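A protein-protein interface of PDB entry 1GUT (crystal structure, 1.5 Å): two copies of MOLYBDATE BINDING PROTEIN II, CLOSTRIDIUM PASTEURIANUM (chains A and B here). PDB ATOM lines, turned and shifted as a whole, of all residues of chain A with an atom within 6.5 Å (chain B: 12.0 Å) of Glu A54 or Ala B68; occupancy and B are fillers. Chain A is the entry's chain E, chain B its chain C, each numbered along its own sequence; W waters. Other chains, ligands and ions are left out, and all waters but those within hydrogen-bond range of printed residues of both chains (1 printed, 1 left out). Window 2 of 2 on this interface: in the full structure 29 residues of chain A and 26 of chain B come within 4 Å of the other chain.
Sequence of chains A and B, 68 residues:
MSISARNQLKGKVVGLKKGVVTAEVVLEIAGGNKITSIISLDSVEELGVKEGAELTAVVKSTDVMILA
The backbone carbonyl oxygen (O) of Leu B67 sits at hydrogen-bond distance from the backbone NH (N) of Thr A56.
The chain-end carboxylate of Ala B68 is in hydrogen-bond range of the side-chain hydroxyl of Thr A56 (3.0 Å).
The backbone carbonyl oxygen of Leu A55 lies within hydrogen-bond range of the backbone NH of Gly A11.
Among the printed residues, merely in contact across the chains: Leu A27 with Ile B66, Thr A56 with Ile B66, Glu A54 with Ala B68, Leu A47 with Ile B66, Thr A56 with Met B65, Leu A55 with Leu B67, Leu A55 with Ala B68, Leu A55 with Ile B66 and Leu A47 with Ala B68.
Glu A54 touches one residue of chain B.
Printed residues of chain A within 4 Å of Ala B68: Leu A47, Glu A54, Leu A55 and Thr A56.
No residue of chain B comes within 4 Å of Gly A11.
No residue of chain B comes within 4 Å of Val A13.
Printed residues of chain B within 4 Å of Leu A47: Ile B66 (3.6 Å) and Ala B68 (3.98 Å).
No residue of chain B comes within 4 Å of Gly A52.
No residue of chain B comes within 4 Å of Ala A53.
Of chain B, only Ile B66 (3.8 Å), Leu B67 (3.7 Å) and Ala B68 (3.8 Å) come within 4 Å of Leu A55.
Printed residues of chain B within 4 Å of Thr A56: Met B65, Ile B66, Leu B67 and Ala B68.
Printed residues of chain A within 4 Å of Met B65: Thr A56.
Lys A50 touches none of the printed residues of chain B.
Val B64 touches none of the printed residues of chain A.
The nearest residue of chain B that does not touch Glu A54 is Leu B67 (5.4 Å).
The nearest printed residue of chain A that does not touch Ala B68 is Gly A11 (7.0 Å).
Of the 11 printed residues of chain A, 5 touch a printed residue of chain B.
Hydrophobic or aromatic side chains of chain B within 4 Å of the printed part of chain A: Ile B66.
Among the printed residues, 11 pairs touch across the chains.
Among the printed residues, no Asp or Glu carboxylate lies within 4 Å of a Lys or Arg side-chain nitrogen of the other chain.
No position is printed for both chains.
Water W1 bridges OXT of Ala B68 (2.7 Å) and OG1 of Thr A56 (2.7 Å).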
ATOM      1  N   GLY A  11     -23.753  14.201  -1.272  1.00  0.00           N
ATOM      2  CA  GLY A  11     -22.809  14.946  -2.069  1.00  0.00           C
ATOM      3  C   GLY A  11     -22.723  16.392  -1.677  1.00  0.00           C
ATOM      4  O   GLY A  11     -23.383  16.836  -0.736  1.00  0.00           O
ATOM      5  N   LYS A  12     -21.897  17.120  -2.405  1.00  0.00           N
ATOM      6  CA  LYS A  12     -21.723  18.537  -2.140  1.00  0.00           C
ATOM      7  C   LYS A  12     -22.147  19.336  -3.367  1.00  0.00           C
ATOM      8  O   LYS A  12     -21.964  18.919  -4.496  1.00  0.00           O
ATOM      9  CB  LYS A  12     -20.269  18.850  -1.772  1.00  0.00           C
ATOM     10  CG  LYS A  12     -19.280  18.435  -2.853  1.00  0.00           C
ATOM     11  CD  LYS A  12     -17.843  18.926  -2.547  1.00  0.00           C
ATOM     12  CE  LYS A  12     -16.876  18.523  -3.657  1.00  0.00           C
ATOM     13  NZ  LYS A  12     -15.469  18.847  -3.271  1.00  0.00           N
ATOM     14  N   VAL A  13     -22.751  20.488  -3.140  1.00  0.00           N
ATOM     15  CA  VAL A  13     -23.181  21.335  -4.244  1.00  0.00           C
ATOM     16  C   VAL A  13     -22.007  21.946  -4.990  1.00  0.00           C
ATOM     17  O   VAL A  13     -21.190  22.673  -4.402  1.00  0.00           O
ATOM     18  CB  VAL A  13     -24.088  22.471  -3.729  1.00  0.00           C
ATOM     19  CG1 VAL A  13     -24.466  23.409  -4.870  1.00  0.00           C
ATOM     20  CG2 VAL A  13     -25.332  21.891  -3.084  1.00  0.00           C
ATOM     21  N   LEU A  27     -24.771  18.182  -7.797  1.00  0.00           N
ATOM     22  CA  LEU A  27     -24.077  17.623  -6.652  1.00  0.00           C
ATOM     23  C   LEU A  27     -22.935  16.698  -7.062  1.00  0.00           C
ATOM     24  O   LEU A  27     -23.107  15.873  -7.950  1.00  0.00           O
ATOM     25  CB  LEU A  27     -25.049  16.813  -5.789  1.00  0.00           C
ATOM     26  CG  LEU A  27     -26.087  17.577  -4.987  1.00  0.00           C
ATOM     27  CD1 LEU A  27     -27.173  16.636  -4.502  1.00  0.00           C
ATOM     28  CD2 LEU A  27     -25.468  18.252  -3.808  1.00  0.00           C
ATOM     29  N   LEU A  47     -33.798  24.651   2.245  1.00  0.00           N
ATOM     30  CA  LEU A  47     -32.618  23.879   2.631  1.00  0.00           C
ATOM     31  C   LEU A  47     -31.372  24.747   2.708  1.00  0.00           C
ATOM     32  O   LEU A  47     -30.338  24.293   3.173  1.00  0.00           O
ATOM     33  CB  LEU A  47     -32.363  22.767   1.624  1.00  0.00           C
ATOM     34  CG  LEU A  47     -33.417  21.669   1.645  1.00  0.00           C
ATOM     35  CD1 LEU A  47     -33.188  20.737   0.470  1.00  0.00           C
ATOM     36  CD2 LEU A  47     -33.323  20.935   2.966  1.00  0.00           C
ATOM     37  N   LYS A  50     -26.523  26.201  -1.378  1.00  0.00           N
ATOM     38  CA  LYS A  50     -25.498  27.137  -1.822  1.00  0.00           C
ATOM     39  C   LYS A  50     -24.270  26.299  -2.133  1.00  0.00           C
ATOM     40  O   LYS A  50     -24.175  25.147  -1.695  1.00  0.00           O
ATOM     41  CB  LYS A  50     -25.188  28.184  -0.741  1.00  0.00           C
ATOM     42  CG  LYS A  50     -24.565  27.637   0.540  1.00  0.00           C
ATOM     43  CD  LYS A  50     -24.309  28.772   1.555  1.00  0.00           C
ATOM     44  CE  LYS A  50     -23.877  28.256   2.918  1.00  0.00           C
ATOM     45  NZ  LYS A  50     -23.913  29.342   3.951  1.00  0.00           N
ATOM     46  N   GLY A  52     -21.043  24.281  -2.033  1.00  0.00           N
ATOM     47  CA  GLY A  52     -20.403  23.608  -0.919  1.00  0.00           C
ATOM     48  C   GLY A  52     -21.351  22.879   0.018  1.00  0.00           C
ATOM     49  O   GLY A  52     -20.922  22.055   0.815  1.00  0.00           O
ATOM     50  N   ALA A  53     -22.642  23.180  -0.049  1.00  0.00           N
ATOM     51  CA  ALA A  53     -23.560  22.521   0.870  1.00  0.00           C
ATOM     52  C   ALA A  53     -23.579  21.007   0.704  1.00  0.00           C
ATOM     53  O   ALA A  53     -23.515  20.477  -0.411  1.00  0.00           O
ATOM     54  CB  ALA A  53     -24.967  23.096   0.737  1.00  0.00           C
ATOM     55  N   GLU A  54     -23.643  20.322   1.837  1.00  0.00           N
ATOM     56  CA  GLU A  54     -23.732  18.868   1.850  1.00  0.00           C
ATOM     57  C   GLU A  54     -25.204  18.514   1.857  1.00  0.00           C
ATOM     58  O   GLU A  54     -25.938  18.852   2.810  1.00  0.00           O
ATOM     59  CB  GLU A  54     -23.060  18.329   3.099  1.00  0.00           C
ATOM     60  CG  GLU A  54     -21.572  18.575   3.080  1.00  0.00           C
ATOM     61  CD  GLU A  54     -20.862  18.097   4.332  1.00  0.00           C
ATOM     62  OE1 GLU A  54     -21.516  17.890   5.385  1.00  0.00           O
ATOM     63  OE2 GLU A  54     -19.638  17.929   4.257  1.00  0.00           O
ATOM     64  N   LEU A  55     -25.644  17.824   0.806  1.00  0.00           N
ATOM     65  CA  LEU A  55     -27.048  17.453   0.670  1.00  0.00           C
ATOM     66  C   LEU A  55     -27.127  16.031   0.143  1.00  0.00           C
ATOM     67  O   LEU A  55     -26.106  15.427  -0.195  1.00  0.00           O
ATOM     68  CB  LEU A  55     -27.748  18.396  -0.317  1.00  0.00           C
ATOM     69  CG  LEU A  55     -27.732  19.876   0.095  1.00  0.00           C
ATOM     70  CD1 LEU A  55     -28.114  20.794  -1.056  1.00  0.00           C
ATOM     71  CD2 LEU A  55     -28.664  20.082   1.296  1.00  0.00           C
ATOM     72  N   THR A  56     -28.337  15.508   0.056  1.00  0.00           N
ATOM     73  CA  THR A  56     -28.530  14.162  -0.446  1.00  0.00           C
ATOM     74  C   THR A  56     -29.441  14.123  -1.664  1.00  0.00           C
ATOM     75  O   THR A  56     -30.553  14.670  -1.628  1.00  0.00           O
ATOM     76  CB  THR A  56     -29.179  13.313   0.658  1.00  0.00           C
ATOM     77  OG1 THR A  56     -28.368  13.360   1.836  1.00  0.00           O
ATOM     78  CG2 THR A  56     -29.203  11.864   0.251  1.00  0.00           C
ATOM     79  N   VAL B  64     -34.768  13.883  -9.625  1.00  0.00           N
ATOM     80  CA  VAL B  64     -33.847  13.870  -8.480  1.00  0.00           C
ATOM     81  C   VAL B  64     -34.288  14.810  -7.359  1.00  0.00           C
ATOM     82  O   VAL B  64     -34.264  16.021  -7.527  1.00  0.00           O
ATOM     83  CB  VAL B  64     -32.429  14.240  -8.924  1.00  0.00           C
ATOM     84  CG1 VAL B  64     -31.469  14.141  -7.749  1.00  0.00           C
ATOM     85  CG2 VAL B  64     -31.971  13.335 -10.098  1.00  0.00           C
ATOM     86  N   MET B  65     -34.781  14.254  -6.257  1.00  0.00           N
ATOM     87  CA  MET B  65     -35.149  15.087  -5.115  1.00  0.00           C
ATOM     88  C   MET B  65     -33.884  15.441  -4.339  1.00  0.00           C
ATOM     89  O   MET B  65     -32.881  14.727  -4.388  1.00  0.00           O
ATOM     90  CB  MET B  65     -36.095  14.366  -4.188  1.00  0.00           C
ATOM     91  CG  MET B  65     -37.433  14.181  -4.783  1.00  0.00           C
ATOM     92  SD  MET B  65     -38.510  13.479  -3.586  1.00  0.00           S
ATOM     93  CE  MET B  65     -38.785  14.872  -2.538  1.00  0.00           C
ATOM     94  N   ILE B  66     -33.909  16.575  -3.660  1.00  0.00           N
ATOM     95  CA  ILE B  66     -32.776  16.978  -2.829  1.00  0.00           C
ATOM     96  C   ILE B  66     -33.305  17.088  -1.403  1.00  0.00           C
ATOM     97  O   ILE B  66     -34.329  17.742  -1.159  1.00  0.00           O
ATOM     98  CB  ILE B  66     -32.156  18.336  -3.279  1.00  0.00           C
ATOM     99  CG1 ILE B  66     -31.539  18.222  -4.684  1.00  0.00           C
ATOM    100  CG2 ILE B  66     -31.102  18.790  -2.258  1.00  0.00           C
ATOM    101  CD1 ILE B  66     -30.378  17.258  -4.781  1.00  0.00           C
ATOM    102  N   LEU B  67     -32.640  16.404  -0.476  1.00  0.00           N
ATOM    103  CA  LEU B  67     -33.005  16.465   0.941  1.00  0.00           C
ATOM    104  C   LEU B  67     -31.756  16.832   1.716  1.00  0.00           C
ATOM    105  O   LEU B  67     -30.652  16.773   1.195  1.00  0.00           O
ATOM    106  CB  LEU B  67     -33.544  15.116   1.439  1.00  0.00           C
ATOM    107  CG  LEU B  67     -34.899  14.607   0.936  1.00  0.00           C
ATOM    108  CD1 LEU B  67     -35.260  13.293   1.651  1.00  0.00           C
ATOM    109  CD2 LEU B  67     -35.990  15.636   1.113  1.00  0.00           C
ATOM    110  N   ALA B  68     -31.927  17.212   2.975  1.00  0.00           N
ATOM    111  CA  ALA B  68     -30.782  17.579   3.789  1.00  0.00           C
ATOM    112  C   ALA B  68     -29.719  16.485   3.783  1.00  0.00           C
ATOM    113  O   ALA B  68     -29.980  15.299   3.529  1.00  0.00           O
ATOM    114  CB  ALA B  68     -31.223  17.881   5.219  1.00  0.00           C
ATOM    115  OXT ALA B  68     -28.544  16.772   4.046  1.00  0.00           O
HETATM  116  O   HOH W   1     -26.684  14.995   3.268  1.00  0.00           O
